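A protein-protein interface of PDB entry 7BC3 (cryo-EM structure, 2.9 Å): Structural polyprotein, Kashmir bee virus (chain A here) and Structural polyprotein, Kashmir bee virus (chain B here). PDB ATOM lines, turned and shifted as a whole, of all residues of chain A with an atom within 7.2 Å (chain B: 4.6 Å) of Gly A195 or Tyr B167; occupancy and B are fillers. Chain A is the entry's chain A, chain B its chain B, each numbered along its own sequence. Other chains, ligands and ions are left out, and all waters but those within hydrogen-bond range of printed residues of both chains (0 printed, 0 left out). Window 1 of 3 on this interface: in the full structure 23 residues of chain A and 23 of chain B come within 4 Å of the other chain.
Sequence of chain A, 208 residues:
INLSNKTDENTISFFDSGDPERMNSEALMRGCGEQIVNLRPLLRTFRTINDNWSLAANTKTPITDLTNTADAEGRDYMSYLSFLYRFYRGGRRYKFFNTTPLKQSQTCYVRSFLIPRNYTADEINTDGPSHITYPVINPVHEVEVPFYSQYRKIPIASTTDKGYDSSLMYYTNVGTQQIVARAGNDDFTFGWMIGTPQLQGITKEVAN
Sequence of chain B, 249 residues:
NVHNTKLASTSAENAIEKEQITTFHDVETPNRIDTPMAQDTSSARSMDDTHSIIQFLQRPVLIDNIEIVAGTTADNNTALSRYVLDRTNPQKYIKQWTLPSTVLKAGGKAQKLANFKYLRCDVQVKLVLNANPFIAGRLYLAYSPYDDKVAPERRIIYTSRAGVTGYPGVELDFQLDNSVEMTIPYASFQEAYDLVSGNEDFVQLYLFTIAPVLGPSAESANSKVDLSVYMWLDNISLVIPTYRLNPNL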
ATOM      1  N   PHE A  83      26.270   4.851 -16.332  1.00  0.00           N
ATOM      2  CA  PHE A  83      26.940   4.964 -17.618  1.00  0.00           C
ATOM      3  C   PHE A  83      27.551   3.649 -18.080  1.00  0.00           C
ATOM      4  O   PHE A  83      28.045   3.580 -19.210  1.00  0.00           O
ATOM      5  CB  PHE A  83      28.021   6.037 -17.537  1.00  0.00           C
ATOM      6  CG  PHE A  83      27.490   7.435 -17.617  1.00  0.00           C
ATOM      7  CD1 PHE A  83      27.256   8.033 -18.840  1.00  0.00           C
ATOM      8  CD2 PHE A  83      27.219   8.151 -16.466  1.00  0.00           C
ATOM      9  CE1 PHE A  83      26.767   9.317 -18.912  1.00  0.00           C
ATOM     10  CE2 PHE A  83      26.731   9.435 -16.534  1.00  0.00           C
ATOM     11  CZ  PHE A  83      26.503  10.019 -17.759  1.00  0.00           C
ATOM     12  N   LEU A  84      27.529   2.617 -17.240  1.00  0.00           N
ATOM     13  CA  LEU A  84      27.988   1.289 -17.614  1.00  0.00           C
ATOM     14  C   LEU A  84      26.854   0.371 -18.031  1.00  0.00           C
ATOM     15  O   LEU A  84      27.120  -0.725 -18.537  1.00  0.00           O
ATOM     16  CB  LEU A  84      28.721   0.628 -16.445  1.00  0.00           C
ATOM     17  CG  LEU A  84      30.172   0.989 -16.173  1.00  0.00           C
ATOM     18  CD1 LEU A  84      30.642   0.183 -14.989  1.00  0.00           C
ATOM     19  CD2 LEU A  84      31.038   0.720 -17.377  1.00  0.00           C
ATOM     20  N   TYR A  85      25.608   0.781 -17.825  1.00  0.00           N
ATOM     21  CA  TYR A  85      24.467  -0.094 -18.017  1.00  0.00           C
ATOM     22  C   TYR A  85      23.406   0.628 -18.831  1.00  0.00           C
ATOM     23  O   TYR A  85      23.517   1.819 -19.132  1.00  0.00           O
ATOM     24  CB  TYR A  85      23.890  -0.557 -16.676  1.00  0.00           C
ATOM     25  CG  TYR A  85      24.896  -1.229 -15.767  1.00  0.00           C
ATOM     26  CD1 TYR A  85      25.052  -2.604 -15.769  1.00  0.00           C
ATOM     27  CD2 TYR A  85      25.679  -0.488 -14.900  1.00  0.00           C
ATOM     28  CE1 TYR A  85      25.959  -3.220 -14.949  1.00  0.00           C
ATOM     29  CE2 TYR A  85      26.592  -1.098 -14.072  1.00  0.00           C
ATOM     30  CZ  TYR A  85      26.728  -2.465 -14.103  1.00  0.00           C
ATOM     31  OH  TYR A  85      27.635  -3.086 -13.280  1.00  0.00           O
ATOM     32  N   ARG A  86      22.369  -0.120 -19.181  1.00  0.00           N
ATOM     33  CA  ARG A  86      21.274   0.364 -20.004  1.00  0.00           C
ATOM     34  C   ARG A  86      19.913   0.235 -19.342  1.00  0.00           C
ATOM     35  O   ARG A  86      18.971   0.904 -19.768  1.00  0.00           O
ATOM     36  CB  ARG A  86      21.254  -0.401 -21.331  1.00  0.00           C
ATOM     37  CG  ARG A  86      22.284   0.053 -22.327  1.00  0.00           C
ATOM     38  CD  ARG A  86      21.938   1.400 -22.900  1.00  0.00           C
ATOM     39  NE  ARG A  86      22.660   1.658 -24.141  1.00  0.00           N
ATOM     40  CZ  ARG A  86      23.736   2.428 -24.246  1.00  0.00           C
ATOM     41  NH1 ARG A  86      24.244   3.037 -23.186  1.00  0.00           N
ATOM     42  NH2 ARG A  86      24.311   2.593 -25.427  1.00  0.00           N
ATOM     43  N   MET A 193      25.672  -4.951 -19.034  1.00  0.00           N
ATOM     44  CA  MET A 193      26.959  -4.296 -18.923  1.00  0.00           C
ATOM     45  C   MET A 193      27.438  -3.915 -20.316  1.00  0.00           C
ATOM     46  O   MET A 193      27.514  -4.764 -21.211  1.00  0.00           O
ATOM     47  CB  MET A 193      27.962  -5.212 -18.237  1.00  0.00           C
ATOM     48  CG  MET A 193      29.058  -4.475 -17.510  1.00  0.00           C
ATOM     49  SD  MET A 193      30.191  -5.622 -16.724  1.00  0.00           S
ATOM     50  CE  MET A 193      30.811  -6.475 -18.165  1.00  0.00           C
ATOM     51  N   ILE A 194      27.751  -2.636 -20.499  1.00  0.00           N
ATOM     52  CA  ILE A 194      28.200  -2.099 -21.770  1.00  0.00           C
ATOM     53  C   ILE A 194      29.540  -1.410 -21.547  1.00  0.00           C
ATOM     54  O   ILE A 194      30.095  -1.423 -20.450  1.00  0.00           O
ATOM     55  CB  ILE A 194      27.182  -1.119 -22.391  1.00  0.00           C
ATOM     56  CG1 ILE A 194      26.773  -0.062 -21.371  1.00  0.00           C
ATOM     57  CG2 ILE A 194      25.966  -1.859 -22.915  1.00  0.00           C
ATOM     58  CD1 ILE A 194      26.371   1.237 -21.988  1.00  0.00           C
ATOM     59  N   GLY A 195      30.055  -0.809 -22.608  1.00  0.00           N
ATOM     60  CA  GLY A 195      31.323  -0.126 -22.530  1.00  0.00           C
ATOM     61  C   GLY A 195      31.243   1.157 -21.732  1.00  0.00           C
ATOM     62  O   GLY A 195      30.177   1.640 -21.347  1.00  0.00           O
ATOM     63  N   THR A 196      32.409   1.711 -21.483  1.00  0.00           N
ATOM     64  CA  THR A 196      32.570   2.900 -20.669  1.00  0.00           C
ATOM     65  C   THR A 196      32.510   4.155 -21.525  1.00  0.00           C
ATOM     66  O   THR A 196      32.804   4.121 -22.723  1.00  0.00           O
ATOM     67  CB  THR A 196      33.907   2.852 -19.938  1.00  0.00           C
ATOM     68  OG1 THR A 196      34.973   2.888 -20.892  1.00  0.00           O
ATOM     69  CG2 THR A 196      34.022   1.590 -19.124  1.00  0.00           C
ATOM     70  N   PRO A 197      32.125   5.289 -20.937  1.00  0.00           N
ATOM     71  CA  PRO A 197      32.326   6.569 -21.620  1.00  0.00           C
ATOM     72  C   PRO A 197      33.671   7.175 -21.266  1.00  0.00           C
ATOM     73  O   PRO A 197      34.425   6.604 -20.473  1.00  0.00           O
ATOM     74  CB  PRO A 197      31.164   7.418 -21.104  1.00  0.00           C
ATOM     75  CG  PRO A 197      30.935   6.914 -19.731  1.00  0.00           C
ATOM     76  CD  PRO A 197      31.360   5.461 -19.691  1.00  0.00           C
ATOM     77  N   TYR B 140      35.386  -5.100 -35.288  1.00  0.00           N
ATOM     78  CA  TYR B 140      34.646  -5.376 -34.065  1.00  0.00           C
ATOM     79  C   TYR B 140      33.165  -5.171 -34.335  1.00  0.00           C
ATOM     80  O   TYR B 140      32.742  -4.073 -34.713  1.00  0.00           O
ATOM     81  CB  TYR B 140      35.109  -4.480 -32.917  1.00  0.00           C
ATOM     82  CG  TYR B 140      34.695  -4.989 -31.556  1.00  0.00           C
ATOM     83  CD1 TYR B 140      35.178  -6.194 -31.069  1.00  0.00           C
ATOM     84  CD2 TYR B 140      33.819  -4.269 -30.761  1.00  0.00           C
ATOM     85  CE1 TYR B 140      34.802  -6.665 -29.830  1.00  0.00           C
ATOM     86  CE2 TYR B 140      33.436  -4.732 -29.521  1.00  0.00           C
ATOM     87  CZ  TYR B 140      33.931  -5.929 -29.059  1.00  0.00           C
ATOM     88  OH  TYR B 140      33.556  -6.394 -27.822  1.00  0.00           O
ATOM     89  N   ALA B 142      29.563  -5.036 -32.681  1.00  0.00           N
ATOM     90  CA  ALA B 142      28.995  -4.774 -31.370  1.00  0.00           C
ATOM     91  C   ALA B 142      27.571  -4.264 -31.521  1.00  0.00           C
ATOM     92  O   ALA B 142      27.214  -3.673 -32.543  1.00  0.00           O
ATOM     93  CB  ALA B 142      29.834  -3.752 -30.597  1.00  0.00           C
ATOM     94  N   TYR B 143      26.761  -4.497 -30.491  1.00  0.00           N
ATOM     95  CA  TYR B 143      25.393  -4.004 -30.440  1.00  0.00           C
ATOM     96  C   TYR B 143      25.216  -3.114 -29.219  1.00  0.00           C
ATOM     97  O   TYR B 143      25.724  -3.417 -28.136  1.00  0.00           O
ATOM     98  CB  TYR B 143      24.375  -5.154 -30.415  1.00  0.00           C
ATOM     99  CG  TYR B 143      24.324  -5.965 -29.137  1.00  0.00           C
ATOM    100  CD1 TYR B 143      24.972  -7.187 -29.043  1.00  0.00           C
ATOM    101  CD2 TYR B 143      23.604  -5.523 -28.036  1.00  0.00           C
ATOM    102  CE1 TYR B 143      24.918  -7.935 -27.885  1.00  0.00           C
ATOM    103  CE2 TYR B 143      23.548  -6.263 -26.876  1.00  0.00           C
ATOM    104  CZ  TYR B 143      24.205  -7.468 -26.806  1.00  0.00           C
ATOM    105  OH  TYR B 143      24.148  -8.209 -25.649  1.00  0.00           O
ATOM    106  N   SER B 144      24.494  -2.013 -29.408  1.00  0.00           N
ATOM    107  CA  SER B 144      24.245  -1.037 -28.358  1.00  0.00           C
ATOM    108  C   SER B 144      22.743  -0.863 -28.176  1.00  0.00           C
ATOM    109  O   SER B 144      22.074  -0.346 -29.087  1.00  0.00           O
ATOM    110  CB  SER B 144      24.895   0.300 -28.702  1.00  0.00           C
ATOM    111  OG  SER B 144      24.735   1.228 -27.646  1.00  0.00           O
ATOM    112  N   ARG B 154      26.086   8.649 -23.710  1.00  0.00           N
ATOM    113  CA  ARG B 154      25.930   7.238 -23.394  1.00  0.00           C
ATOM    114  C   ARG B 154      25.918   6.356 -24.631  1.00  0.00           C
ATOM    115  O   ARG B 154      25.720   5.143 -24.509  1.00  0.00           O
ATOM    116  CB  ARG B 154      24.636   7.018 -22.610  1.00  0.00           C
ATOM    117  CG  ARG B 154      24.507   7.858 -21.366  1.00  0.00           C
ATOM    118  CD  ARG B 154      23.154   7.666 -20.726  1.00  0.00           C
ATOM    119  NE  ARG B 154      23.119   8.168 -19.357  1.00  0.00           N
ATOM    120  CZ  ARG B 154      23.416   7.445 -18.283  1.00  0.00           C
ATOM    121  NH1 ARG B 154      23.781   6.178 -18.407  1.00  0.00           N
ATOM    122  NH2 ARG B 154      23.355   7.992 -17.080  1.00  0.00           N
ATOM    123  N   ARG B 155      26.120   6.927 -25.814  1.00  0.00           N
ATOM    124  CA  ARG B 155      26.088   6.152 -27.041  1.00  0.00           C
ATOM    125  C   ARG B 155      27.419   5.447 -27.265  1.00  0.00           C
ATOM    126  O   ARG B 155      28.473   5.880 -26.791  1.00  0.00           O
ATOM    127  CB  ARG B 155      25.770   7.052 -28.232  1.00  0.00           C
ATOM    128  CG  ARG B 155      24.360   7.604 -28.226  1.00  0.00           C
ATOM    129  CD  ARG B 155      24.133   8.573 -29.369  1.00  0.00           C
ATOM    130  NE  ARG B 155      24.027   7.894 -30.656  1.00  0.00           N
ATOM    131  CZ  ARG B 155      23.684   8.498 -31.790  1.00  0.00           C
ATOM    132  NH1 ARG B 155      23.412   9.795 -31.800  1.00  0.00           N
ATOM    133  NH2 ARG B 155      23.612   7.801 -32.914  1.00  0.00           N
ATOM    134  N   ILE B 156      27.359   4.336 -28.001  1.00  0.00           N
ATOM    135  CA  ILE B 156      28.587   3.668 -28.408  1.00  0.00           C
ATOM    136  C   ILE B 156      29.366   4.558 -29.361  1.00  0.00           C
ATOM    137  O   ILE B 156      30.602   4.543 -29.370  1.00  0.00           O
ATOM    138  CB  ILE B 156      28.270   2.299 -29.031  1.00  0.00           C
ATOM    139  CG1 ILE B 156      29.539   1.457 -29.125  1.00  0.00           C
ATOM    140  CG2 ILE B 156      27.635   2.473 -30.392  1.00  0.00           C
ATOM    141  CD1 ILE B 156      29.300   0.070 -29.643  1.00  0.00           C
ATOM    142  N   GLY B 163      35.978   2.090 -24.751  1.00  0.00           N
ATOM    143  CA  GLY B 163      34.568   1.932 -24.450  1.00  0.00           C
ATOM    144  C   GLY B 163      33.857   1.086 -25.487  1.00  0.00           C
ATOM    145  O   GLY B 163      33.145   0.138 -25.152  1.00  0.00           O
ATOM    146  N   VAL B 164      34.053   1.415 -26.764  1.00  0.00           N
ATOM    147  CA  VAL B 164      33.444   0.634 -27.840  1.00  0.00           C
ATOM    148  C   VAL B 164      33.752  -0.844 -27.657  1.00  0.00           C
ATOM    149  O   VAL B 164      32.851  -1.690 -27.631  1.00  0.00           O
ATOM    150  CB  VAL B 164      33.928   1.143 -29.209  1.00  0.00           C
ATOM    151  CG1 VAL B 164      33.353   0.292 -30.317  1.00  0.00           C
ATOM    152  CG2 VAL B 164      33.548   2.599 -29.402  1.00  0.00           C
ATOM    153  N   THR B 165      35.036  -1.179 -27.529  1.00  0.00           N
ATOM    154  CA  THR B 165      35.430  -2.565 -27.327  1.00  0.00           C
ATOM    155  C   THR B 165      34.961  -3.119 -25.991  1.00  0.00           C
ATOM    156  O   THR B 165      35.019  -4.336 -25.789  1.00  0.00           O
ATOM    157  CB  THR B 165      36.945  -2.694 -27.438  1.00  0.00           C
ATOM    158  OG1 THR B 165      37.576  -1.776 -26.539  1.00  0.00           O
ATOM    159  CG2 THR B 165      37.386  -2.391 -28.853  1.00  0.00           C
ATOM    160  N   GLY B 166      34.503  -2.264 -25.080  1.00  0.00           N
ATOM    161  CA  GLY B 166      33.866  -2.734 -23.869  1.00  0.00           C
ATOM    162  C   GLY B 166      32.427  -3.150 -24.042  1.00  0.00           C
ATOM    163  O   GLY B 166      31.866  -3.791 -23.149  1.00  0.00           O
ATOM    164  N   TYR B 167      31.816  -2.799 -25.168  1.00  0.00           N
ATOM    165  CA  TYR B 167      30.479  -3.260 -25.479  1.00  0.00           C
ATOM    166  C   TYR B 167      30.511  -4.728 -25.883  1.00  0.00           C
ATOM    167  O   TYR B 167      31.553  -5.250 -26.290  1.00  0.00           O
ATOM    168  CB  TYR B 167      29.880  -2.428 -26.608  1.00  0.00           C
ATOM    169  CG  TYR B 167      29.329  -1.092 -26.174  1.00  0.00           C
ATOM    170  CD1 TYR B 167      27.966  -0.846 -26.190  1.00  0.00           C
ATOM    171  CD2 TYR B 167      30.171  -0.075 -25.759  1.00  0.00           C
ATOM    172  CE1 TYR B 167      27.458   0.372 -25.797  1.00  0.00           C
ATOM    173  CE2 TYR B 167      29.672   1.146 -25.363  1.00  0.00           C
ATOM    174  CZ  TYR B 167      28.315   1.365 -25.385  1.00  0.00           C
ATOM    175  OH  TYR B 167      27.813   2.581 -24.991  1.00  0.00           O
ATOM    176  N   PRO B 168      29.383  -5.424 -25.775  1.00  0.00           N
ATOM    177  CA  PRO B 168      29.342  -6.823 -26.212  1.00  0.00           C
ATOM    178  C   PRO B 168      29.569  -6.932 -27.711  1.00  0.00           C
ATOM    179  O   PRO B 168      28.888  -6.285 -28.509  1.00  0.00           O
ATOM    180  CB  PRO B 168      27.935  -7.279 -25.812  1.00  0.00           C
ATOM    181  CG  PRO B 168      27.149  -6.029 -25.669  1.00  0.00           C
ATOM    182  CD  PRO B 168      28.097  -4.981 -25.214  1.00  0.00           C
ATOM    183  N   GLY B 169      30.534  -7.761 -28.090  1.00  0.00           N
ATOM    184  CA  GLY B 169      30.877  -7.891 -29.492  1.00  0.00           C
ATOM    185  C   GLY B 169      31.816  -9.054 -29.714  1.00  0.00           C
ATOM    186  O   GLY B 169      32.175  -9.783 -28.786  1.00  0.00           O
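Among the printed residues, merely in contact across the chains: Gly A195 with Gly B163, Gly A195 with Tyr B167, Thr A196 with Gly B163, Phe A83 with Arg B154, Arg A86 with Tyr B167, Gly A195 with Gly B166, Ile A194 with Tyr B167 and Ile A194 with Gly B166.
Of the 9 printed residues of chain A, 5 touch a printed residue of chain B.
Among the printed residues, 10 pairs touch across the chains.
Among the printed residues, no Asp or Glu carboxylate lies within 4 Å of a Lys or Arg side-chain nitrogen of the other chain.
The side-chain hydroxyl (OG) of Ser B144 lies within hydrogen-bond range of the guanidinium group (NH2) of Arg A86 (2.6 Å).
The backbone carbonyl oxygen (O) of Arg B154 sits at hydrogen-bond distance from the guanidinium group (NH1) of Arg A86, at 2.9 Å.
The side-chain hydroxyl (OH) of Tyr B140 lies within hydrogen-bond range of the backbone carbonyl oxygen (O) of Tyr B167 (2.8 Å).
The side-chain hydroxyl of Tyr B167 lies within hydrogen-bond range of the backbone carbonyl oxygen of Arg B154 (3.3 Å).
The backbone carbonyl oxygen (O) of Leu A84 sits at hydrogen-bond distance from the backbone NH (N) of Ile A194 (2.8 Å).
Printed residues of chain B within 4 Å of Phe A83: Arg B154.
Tyr B140 touches none of the printed residues of chain A.
Printed residues of chain A within 4 Å of Arg B154: Phe A83 (3.5 Å) and Arg A86 (2.9 Å).
Of chain A, only Arg A86, Ile A194 and Gly A195 come within 4 Å of Tyr B167.
The nearest printed residue of chain A that does not touch Arg B154 is Tyr A85 (4.4 Å).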
